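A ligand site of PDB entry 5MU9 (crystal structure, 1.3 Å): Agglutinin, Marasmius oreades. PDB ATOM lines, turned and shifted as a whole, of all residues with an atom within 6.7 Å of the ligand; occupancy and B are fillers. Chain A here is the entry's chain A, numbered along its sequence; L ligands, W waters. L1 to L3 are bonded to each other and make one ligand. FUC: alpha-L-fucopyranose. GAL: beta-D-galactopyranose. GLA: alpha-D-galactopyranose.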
ATOM      1  N   HIS A   9     -20.566 -11.341 -31.960  1.00  0.00           N
ATOM      2  CA  HIS A   9     -21.436 -10.191 -31.887  1.00  0.00           C
ATOM      3  C   HIS A   9     -22.142 -10.153 -33.249  1.00  0.00           C
ATOM      4  O   HIS A   9     -21.439 -10.116 -34.268  1.00  0.00           O
ATOM      5  CB  HIS A   9     -20.544  -8.957 -31.645  1.00  0.00           C
ATOM      6  CG  HIS A   9     -21.338  -7.731 -31.410  1.00  0.00           C
ATOM      7  ND1 HIS A   9     -21.466  -6.699 -32.320  1.00  0.00           N
ATOM      8  CD2 HIS A   9     -22.075  -7.410 -30.329  1.00  0.00           C
ATOM      9  CE1 HIS A   9     -22.271  -5.815 -31.811  1.00  0.00           C
ATOM     10  NE2 HIS A   9     -22.585  -6.188 -30.578  1.00  0.00           N
ATOM     11  N   ASP A  20     -29.680  -8.658 -29.426  1.00  0.00           N
ATOM     12  CA  ASP A  20     -29.523  -8.324 -28.024  1.00  0.00           C
ATOM     13  C   ASP A  20     -30.576  -9.102 -27.240  1.00  0.00           C
ATOM     14  O   ASP A  20     -31.796  -9.014 -27.514  1.00  0.00           O
ATOM     15  CB  ASP A  20     -29.691  -6.813 -27.886  1.00  0.00           C
ATOM     16  CG  ASP A  20     -29.509  -6.269 -26.434  1.00  0.00           C
ATOM     17  OD1 ASP A  20     -30.324  -6.658 -25.584  1.00  0.00           O
ATOM     18  OD2 ASP A  20     -28.628  -5.395 -26.250  1.00  0.00           O
ATOM     19  N   LEU A  21     -30.165  -9.826 -26.200  1.00  0.00           N
ATOM     20  CA  LEU A  21     -31.142 -10.467 -25.305  1.00  0.00           C
ATOM     21  C   LEU A  21     -31.535  -9.440 -24.265  1.00  0.00           C
ATOM     22  O   LEU A  21     -30.690  -8.935 -23.462  1.00  0.00           O
ATOM     23  CB  LEU A  21     -30.484 -11.677 -24.617  1.00  0.00           C
ATOM     24  CG  LEU A  21     -31.405 -12.343 -23.643  1.00  0.00           C
ATOM     25  CD1 LEU A  21     -32.659 -12.993 -24.262  1.00  0.00           C
ATOM     26  CD2 LEU A  21     -30.644 -13.466 -22.906  1.00  0.00           C
ATOM     27  N   LYS A  22     -32.783  -9.003 -24.296  1.00  0.00           N
ATOM     28  CA  LYS A  22     -33.219  -7.798 -23.580  1.00  0.00           C
ATOM     29  C   LYS A  22     -32.921  -7.893 -22.073  1.00  0.00           C
ATOM     30  O   LYS A  22     -33.372  -8.797 -21.397  1.00  0.00           O
ATOM     31  CB  LYS A  22     -34.694  -7.502 -23.857  1.00  0.00           C
ATOM     32  CG  LYS A  22     -34.990  -6.064 -23.606  1.00  0.00           C
ATOM     33  CD  LYS A  22     -36.448  -5.677 -24.042  1.00  0.00           C
ATOM     34  CE  LYS A  22     -36.677  -4.213 -23.761  1.00  0.00           C
ATOM     35  NZ  LYS A  22     -38.028  -3.760 -24.274  1.00  0.00           N
ATOM     36  N   ASP A  23     -32.199  -6.871 -21.613  1.00  0.00           N
ATOM     37  CA  ASP A  23     -31.748  -6.774 -20.208  1.00  0.00           C
ATOM     38  C   ASP A  23     -30.858  -7.923 -19.766  1.00  0.00           C
ATOM     39  O   ASP A  23     -30.644  -8.096 -18.528  1.00  0.00           O
ATOM     40  CB  ASP A  23     -32.938  -6.579 -19.236  1.00  0.00           C
ATOM     41  CG  ASP A  23     -32.562  -5.850 -17.940  1.00  0.00           C
ATOM     42  OD1 ASP A  23     -31.733  -4.939 -18.022  1.00  0.00           O
ATOM     43  OD2 ASP A  23     -33.118  -6.210 -16.851  1.00  0.00           O
ATOM     44  N   GLY A  24     -30.385  -8.729 -20.711  1.00  0.00           N
ATOM     45  CA  GLY A  24     -29.630  -9.917 -20.339  1.00  0.00           C
ATOM     46  C   GLY A  24     -30.414 -10.950 -19.532  1.00  0.00           C
ATOM     47  O   GLY A  24     -29.798 -11.777 -18.892  1.00  0.00           O
ATOM     48  N   VAL A  33     -33.944  -8.728 -29.345  1.00  0.00           N
ATOM     49  CA  VAL A  33     -34.249  -7.421 -30.001  1.00  0.00           C
ATOM     50  C   VAL A  33     -33.048  -6.853 -30.691  1.00  0.00           C
ATOM     51  O   VAL A  33     -31.886  -7.170 -30.352  1.00  0.00           O
ATOM     52  CB  VAL A  33     -34.864  -6.417 -29.019  1.00  0.00           C
ATOM     53  CG1 VAL A  33     -36.205  -6.921 -28.427  1.00  0.00           C
ATOM     54  CG2 VAL A  33     -33.861  -6.102 -27.881  1.00  0.00           C
ATOM     55  N   TRP A  35     -30.509  -3.712 -31.058  1.00  0.00           N
ATOM     56  CA  TRP A  35     -30.053  -2.635 -30.104  1.00  0.00           C
ATOM     57  C   TRP A  35     -28.714  -2.111 -30.599  1.00  0.00           C
ATOM     58  O   TRP A  35     -27.857  -2.869 -31.062  1.00  0.00           O
ATOM     59  CB  TRP A  35     -29.938  -3.250 -28.680  1.00  0.00           C
ATOM     60  CG  TRP A  35     -30.056  -2.253 -27.549  1.00  0.00           C
ATOM     61  CD1 TRP A  35     -29.160  -1.303 -27.116  1.00  0.00           C
ATOM     62  CD2 TRP A  35     -31.229  -2.069 -26.781  1.00  0.00           C
ATOM     63  NE1 TRP A  35     -29.704  -0.515 -26.095  1.00  0.00           N
ATOM     64  CE2 TRP A  35     -30.972  -0.981 -25.873  1.00  0.00           C
ATOM     65  CE3 TRP A  35     -32.470  -2.692 -26.731  1.00  0.00           C
ATOM     66  CZ2 TRP A  35     -31.959  -0.566 -24.959  1.00  0.00           C
ATOM     67  CZ3 TRP A  35     -33.415  -2.238 -25.890  1.00  0.00           C
ATOM     68  CH2 TRP A  35     -33.148  -1.246 -24.991  1.00  0.00           C
ATOM     69  N   GLN A  36     -28.494  -0.831 -30.402  1.00  0.00           N
ATOM     70  CA  GLN A  36     -27.181  -0.218 -30.766  1.00  0.00           C
ATOM     71  C   GLN A  36     -26.113  -0.749 -29.882  1.00  0.00           C
ATOM     72  O   GLN A  36     -26.318  -1.312 -28.761  1.00  0.00           O
ATOM     73  CB  GLN A  36     -27.301   1.275 -30.730  1.00  0.00           C
ATOM     74  CG  GLN A  36     -27.424   1.926 -29.316  1.00  0.00           C
ATOM     75  CD  GLN A  36     -27.508   3.386 -29.379  1.00  0.00           C
ATOM     76  OE1 GLN A  36     -26.564   4.040 -29.807  1.00  0.00           O
ATOM     77  NE2 GLN A  36     -28.670   3.905 -29.028  1.00  0.00           N
ATOM     78  N   PHE A  37     -24.857  -0.562 -30.329  1.00  0.00           N
ATOM     79  CA  PHE A  37     -23.705  -1.118 -29.634  1.00  0.00           C
ATOM     80  C   PHE A  37     -22.547  -0.166 -29.680  1.00  0.00           C
ATOM     81  O   PHE A  37     -22.562   0.851 -30.429  1.00  0.00           O
ATOM     82  CB  PHE A  37     -23.325  -2.453 -30.283  1.00  0.00           C
ATOM     83  CG  PHE A  37     -22.883  -2.377 -31.699  1.00  0.00           C
ATOM     84  CD1 PHE A  37     -23.766  -2.514 -32.747  1.00  0.00           C
ATOM     85  CD2 PHE A  37     -21.532  -2.255 -31.995  1.00  0.00           C
ATOM     86  CE1 PHE A  37     -23.361  -2.490 -34.024  1.00  0.00           C
ATOM     87  CE2 PHE A  37     -21.141  -2.223 -33.310  1.00  0.00           C
ATOM     88  CZ  PHE A  37     -22.065  -2.349 -34.278  1.00  0.00           C
ATOM     89  N   THR A  38     -21.502  -0.468 -28.859  1.00  0.00           N
ATOM     90  CA  THR A  38     -20.317   0.403 -28.843  1.00  0.00           C
ATOM     91  C   THR A  38     -19.164  -0.492 -29.287  1.00  0.00           C
ATOM     92  O   THR A  38     -18.848  -1.517 -28.605  1.00  0.00           O
ATOM     93  CB  THR A  38     -20.072   0.999 -27.421  1.00  0.00           C
ATOM     94  OG1 THR A  38     -21.262   1.657 -26.967  1.00  0.00           O
ATOM     95  CG2 THR A  38     -18.897   1.911 -27.482  1.00  0.00           C
ATOM     96  N   PRO A  39     -18.455  -0.186 -30.358  1.00  0.00           N
ATOM     97  CA  PRO A  39     -17.329  -0.997 -30.799  1.00  0.00           C
ATOM     98  C   PRO A  39     -16.215  -0.975 -29.782  1.00  0.00           C
ATOM     99  O   PRO A  39     -16.112  -0.030 -29.027  1.00  0.00           O
ATOM    100  CB  PRO A  39     -16.822  -0.347 -32.098  1.00  0.00           C
ATOM    101  CG  PRO A  39     -18.052   0.433 -32.547  1.00  0.00           C
ATOM    102  CD  PRO A  39     -18.699   0.946 -31.303  1.00  0.00           C
ATOM    103  N   THR A  41     -15.790  -2.565 -27.047  1.00  0.00           N
ATOM    104  CA  THR A  41     -16.293  -2.835 -25.664  1.00  0.00           C
ATOM    105  C   THR A  41     -16.756  -4.279 -25.576  1.00  0.00           C
ATOM    106  O   THR A  41     -17.033  -4.954 -26.583  1.00  0.00           O
ATOM    107  CB  THR A  41     -17.433  -1.891 -25.282  1.00  0.00           C
ATOM    108  OG1 THR A  41     -18.646  -2.270 -25.936  1.00  0.00           O
ATOM    109  CG2 THR A  41     -17.095  -0.419 -25.455  1.00  0.00           C
ATOM    110  N   ILE A  42     -16.946  -4.758 -24.328  1.00  0.00           N
ATOM    111  CA  ILE A  42     -17.840  -5.838 -24.089  1.00  0.00           C
ATOM    112  C   ILE A  42     -19.267  -5.339 -24.107  1.00  0.00           C
ATOM    113  O   ILE A  42     -19.706  -4.517 -23.289  1.00  0.00           O
ATOM    114  CB  ILE A  42     -17.502  -6.540 -22.729  1.00  0.00           C
ATOM    115  CG1 ILE A  42     -16.075  -7.170 -22.767  1.00  0.00           C
ATOM    116  CG2 ILE A  42     -18.570  -7.558 -22.404  1.00  0.00           C
ATOM    117  CD1 ILE A  42     -15.815  -8.255 -23.762  1.00  0.00           C
ATOM    118  N   ASN A  43     -20.019  -5.839 -25.117  1.00  0.00           N
ATOM    119  CA  ASN A  43     -21.449  -5.506 -25.230  1.00  0.00           C
ATOM    120  C   ASN A  43     -22.152  -6.645 -24.532  1.00  0.00           C
ATOM    121  O   ASN A  43     -22.405  -7.741 -25.082  1.00  0.00           O
ATOM    122  CB  ASN A  43     -21.866  -5.380 -26.686  1.00  0.00           C
ATOM    123  CG  ASN A  43     -21.331  -4.123 -27.339  1.00  0.00           C
ATOM    124  OD1 ASN A  43     -21.853  -3.054 -27.092  1.00  0.00           O
ATOM    125  ND2 ASN A  43     -20.305  -4.258 -28.132  1.00  0.00           N
ATOM    126  N   TRP A  44     -22.446  -6.412 -23.241  1.00  0.00           N
ATOM    127  CA  TRP A  44     -22.804  -7.422 -22.266  1.00  0.00           C
ATOM    128  C   TRP A  44     -24.004  -8.349 -22.599  1.00  0.00           C
ATOM    129  O   TRP A  44     -24.003  -9.513 -22.205  1.00  0.00           O
ATOM    130  CB  TRP A  44     -23.059  -6.772 -20.870  1.00  0.00           C
ATOM    131  CG  TRP A  44     -21.791  -6.433 -20.192  1.00  0.00           C
ATOM    132  CD1 TRP A  44     -21.169  -5.257 -20.193  1.00  0.00           C
ATOM    133  CD2 TRP A  44     -20.967  -7.326 -19.435  1.00  0.00           C
ATOM    134  NE1 TRP A  44     -20.027  -5.311 -19.465  1.00  0.00           N
ATOM    135  CE2 TRP A  44     -19.843  -6.588 -19.022  1.00  0.00           C
ATOM    136  CE3 TRP A  44     -21.076  -8.636 -19.097  1.00  0.00           C
ATOM    137  CZ2 TRP A  44     -18.859  -7.137 -18.256  1.00  0.00           C
ATOM    138  CZ3 TRP A  44     -20.116  -9.193 -18.382  1.00  0.00           C
ATOM    139  CH2 TRP A  44     -19.001  -8.486 -17.952  1.00  0.00           C
ATOM    140  N   HIS A  45     -25.032  -7.828 -23.336  1.00  0.00           N
ATOM    141  CA  HIS A  45     -26.190  -8.583 -23.621  1.00  0.00           C
ATOM    142  C   HIS A  45     -26.208  -9.116 -25.096  1.00  0.00           C
ATOM    143  O   HIS A  45     -27.234  -9.689 -25.513  1.00  0.00           O
ATOM    144  CB  HIS A  45     -27.465  -7.780 -23.341  1.00  0.00           C
ATOM    145  CG  HIS A  45     -27.499  -7.287 -21.951  1.00  0.00           C
ATOM    146  ND1 HIS A  45     -28.268  -6.211 -21.583  1.00  0.00           N
ATOM    147  CD2 HIS A  45     -26.920  -7.719 -20.803  1.00  0.00           C
ATOM    148  CE1 HIS A  45     -28.158  -5.986 -20.286  1.00  0.00           C
ATOM    149  NE2 HIS A  45     -27.330  -6.895 -19.776  1.00  0.00           N
ATOM    150  N   GLN A  46     -25.064  -8.934 -25.802  1.00  0.00           N
ATOM    151  CA  GLN A  46     -25.037  -9.085 -27.268  1.00  0.00           C
ATOM    152  C   GLN A  46     -23.980 -10.095 -27.714  1.00  0.00           C
ATOM    153  O   GLN A  46     -23.539 -10.016 -28.851  1.00  0.00           O
ATOM    154  CB  GLN A  46     -24.784  -7.712 -27.908  1.00  0.00           C
ATOM    155  CG  GLN A  46     -25.835  -6.662 -27.574  1.00  0.00           C
ATOM    156  CD  GLN A  46     -25.569  -5.283 -28.157  1.00  0.00           C
ATOM    157  OE1 GLN A  46     -24.492  -5.044 -28.746  1.00  0.00           O
ATOM    158  NE2 GLN A  46     -26.479  -4.332 -27.892  1.00  0.00           N
ATOM    159  N   PHE A  66     -24.017 -14.045 -21.562  1.00  0.00           N
ATOM    160  CA  PHE A  66     -24.380 -13.531 -20.244  1.00  0.00           C
ATOM    161  C   PHE A  66     -25.469 -14.348 -19.531  1.00  0.00           C
ATOM    162  O   PHE A  66     -25.256 -14.711 -18.349  1.00  0.00           O
ATOM    163  CB  PHE A  66     -24.782 -12.058 -20.378  1.00  0.00           C
ATOM    164  CG  PHE A  66     -25.159 -11.418 -19.048  1.00  0.00           C
ATOM    165  CD1 PHE A  66     -24.134 -10.985 -18.201  1.00  0.00           C
ATOM    166  CD2 PHE A  66     -26.437 -11.252 -18.686  1.00  0.00           C
ATOM    167  CE1 PHE A  66     -24.428 -10.392 -16.994  1.00  0.00           C
ATOM    168  CE2 PHE A  66     -26.769 -10.593 -17.491  1.00  0.00           C
ATOM    169  CZ  PHE A  66     -25.770 -10.227 -16.630  1.00  0.00           C
ATOM    170  N   ASP A 131     -33.689   1.096 -30.588  1.00  0.00           N
ATOM    171  CA  ASP A 131     -33.297   0.185 -29.528  1.00  0.00           C
ATOM    172  C   ASP A 131     -34.520  -0.567 -29.054  1.00  0.00           C
ATOM    173  O   ASP A 131     -35.547   0.106 -28.595  1.00  0.00           O
ATOM    174  CB  ASP A 131     -32.643   0.907 -28.373  1.00  0.00           C
ATOM    175  CG  ASP A 131     -31.270   1.546 -28.814  1.00  0.00           C
ATOM    176  OD1 ASP A 131     -30.632   1.010 -29.685  1.00  0.00           O
ATOM    177  OD2 ASP A 131     -30.834   2.513 -28.070  1.00  0.00           O
HETATM  178  C1  FUC L   1     -25.315  -1.335 -21.091  1.00  0.00           C
HETATM  179  C2  FUC L   1     -24.830  -0.103 -20.352  1.00  0.00           C
HETATM  180  C3  FUC L   1     -25.168  -0.231 -18.887  1.00  0.00           C
HETATM  181  C4  FUC L   1     -24.631  -1.493 -18.295  1.00  0.00           C
HETATM  182  C5  FUC L   1     -25.210  -2.671 -19.126  1.00  0.00           C
HETATM  183  C6  FUC L   1     -24.772  -4.014 -18.633  1.00  0.00           C
HETATM  184  O2  FUC L   1     -25.487   1.088 -20.924  1.00  0.00           O
HETATM  185  O3  FUC L   1     -24.610   0.968 -18.196  1.00  0.00           O
HETATM  186  O4  FUC L   1     -23.213  -1.519 -18.269  1.00  0.00           O
HETATM  187  O5  FUC L   1     -24.807  -2.537 -20.480  1.00  0.00           O
HETATM  188  C1  GAL L   2     -28.696  -2.442 -21.130  1.00  0.00           C
HETATM  189  C2  GAL L   2     -27.338  -2.398 -21.817  1.00  0.00           C
HETATM  190  C3  GAL L   2     -27.517  -2.126 -23.285  1.00  0.00           C
HETATM  191  C4  GAL L   2     -28.471  -3.082 -23.937  1.00  0.00           C
HETATM  192  C5  GAL L   2     -29.802  -3.092 -23.152  1.00  0.00           C
HETATM  193  C6  GAL L   2     -30.849  -4.070 -23.666  1.00  0.00           C
HETATM  194  O1  GAL L   2     -28.526  -2.905 -19.827  1.00  0.00           O
HETATM  195  O2  GAL L   2     -26.697  -1.277 -21.175  1.00  0.00           O
HETATM  196  O3  GAL L   2     -26.207  -2.100 -23.824  1.00  0.00           O
HETATM  197  O4  GAL L   2     -27.903  -4.390 -23.988  1.00  0.00           O
HETATM  198  O5  GAL L   2     -29.514  -3.425 -21.753  1.00  0.00           O
HETATM  199  O6  GAL L   2     -30.506  -5.425 -23.343  1.00  0.00           O
HETATM  200  C1  GLA L   3     -26.129  -1.808 -25.245  1.00  0.00           C
HETATM  201  C2  GLA L   3     -24.679  -1.746 -25.705  1.00  0.00           C
HETATM  202  C3  GLA L   3     -23.965  -0.501 -25.207  1.00  0.00           C
HETATM  203  C4  GLA L   3     -24.741   0.745 -25.516  1.00  0.00           C
HETATM  204  C5  GLA L   3     -26.133   0.560 -24.893  1.00  0.00           C
HETATM  205  C6  GLA L   3     -27.077   1.726 -25.093  1.00  0.00           C
HETATM  206  O2  GLA L   3     -23.943  -2.907 -25.309  1.00  0.00           O
HETATM  207  O3  GLA L   3     -22.659  -0.373 -25.786  1.00  0.00           O
HETATM  208  O4  GLA L   3     -24.862   0.936 -26.955  1.00  0.00           O
HETATM  209  O5  GLA L   3     -26.757  -0.560 -25.521  1.00  0.00           O
HETATM  210  O6  GLA L   3     -28.355   1.516 -24.465  1.00  0.00           O
HETATM  211  O   HOH W   1     -24.331   0.263 -15.405  1.00  0.00           O
HETATM  212  O   HOH W   2     -21.758  -1.665 -20.633  1.00  0.00           O
HETATM  213  O   HOH W   3     -25.264  -5.168 -24.288  1.00  0.00           O
HETATM  214  O   HOH W   4     -30.613   2.808 -25.330  1.00  0.00           O
HETATM  215  O   HOH W   5     -20.845  -1.770 -24.310  1.00  0.00           O
HETATM  216  O   HOH W   6     -28.199   1.398 -21.646  1.00  0.00           O
HETATM  217  O   HOH W   7     -31.902  -3.251 -20.198  1.00  0.00           O
HETATM  218  O   HOH W   8     -22.564  -3.390 -22.676  1.00  0.00           O
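An oxygen (O6) of GAL L2 sits at hydrogen-bond distance from the side-chain carboxylate of Asp 20 (2.6 Å). O of Gln 36 sits at hydrogen-bond distance from O4 of GLA L3 (3.2 Å). The backbone NH of Thr 38 sits at hydrogen-bond distance from an oxygen (O3) of GLA L3 (3.3 Å). The indole nitrogen of Trp 35 lies within hydrogen-bond range of an oxygen (O6) of GLA L3 (2.9 Å). O6 of GAL L2 is in hydrogen-bond range of ND1 of His 45 (3.0 Å). The side-chain amide oxygen of Asn 43 sits at hydrogen-bond distance from an oxygen (O2) of GLA L3 (2.8 Å). N of Asp 23 is in hydrogen-bond range of O6 of GAL L2 (2.8 Å). The side-chain hydroxyl of Thr 38 sits at hydrogen-bond distance from an oxygen (O3) of GLA L3, 2.7 Å away.
N of Gly 24 lies within hydrogen-bond range of ND1 of His 45 (3.4 Å). O of Thr 38 lies within hydrogen-bond range of OG1 of Thr 41 (2.8 Å). O of Gln 36 sits at hydrogen-bond distance from NE2 of Gln 46 (3.1 Å). The side-chain amide nitrogen (NE2) of Gln 36 sits at hydrogen-bond distance from the side-chain carboxylate (OD2) of Asp 131, 2.7 Å away. The backbone NH (N) of Asp 20 is in hydrogen-bond range of the backbone carbonyl oxygen (O) of Val 33, 2.8 Å away. O of Thr 38 is in hydrogen-bond range of ND2 of Asn 43 (3.1 Å). NE2 of Gln 46 lies within hydrogen-bond range of OD2 of Asp 20, at 2.9 Å. The backbone NH of Leu 21 sits at hydrogen-bond distance from the backbone carbonyl oxygen of His 45 (3.0 Å).
Residues that only touch the ligand: Leu 21, Lys 22, Phe 37, Trp 44 and Gln 46. 12 residues have an atom within 4 Å of the ligand: Asp 20, Leu 21, Lys 22, Asp 23, Trp 35, Gln 36, Phe 37, Thr 38, Asn 43, Trp 44, His 45 and Gln 46. Along chain A the residues within 4 Å of the ligand span positions 20 to 46. The nearest printed residue that does not touch the ligand is Gly 24 (4.2 Å).
Water W5 lies within hydrogen-bond range of an oxygen (O3) of GLA L3, the side-chain hydroxyl of Thr 41, the backbone carbonyl oxygen of Ile 42 and the side-chain amide oxygen of Asn 43. Water W4 lies within hydrogen-bond range of O6 of GLA L3 (2.7 Å) and OD2 of Asp 131 (2.8 Å). Water W3 lies within hydrogen-bond range of O4 of GAL L2 (2.8 Å), N of His 45 (2.8 Å) and N of Trp 44 (3.3 Å). Water W7 bridges the side-chain carboxylate (OD1) of Asp 23 (2.8 Å) and an oxygen (O5) of GAL L2 (2.9 Å). Water W8 lies within hydrogen-bond range of an oxygen (O2) of GLA L3 (3.0 Å), the backbone NH (N) of Trp 44 (3.1 Å) and the backbone carbonyl oxygen (O) of Ile 42 (3.1 Å).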
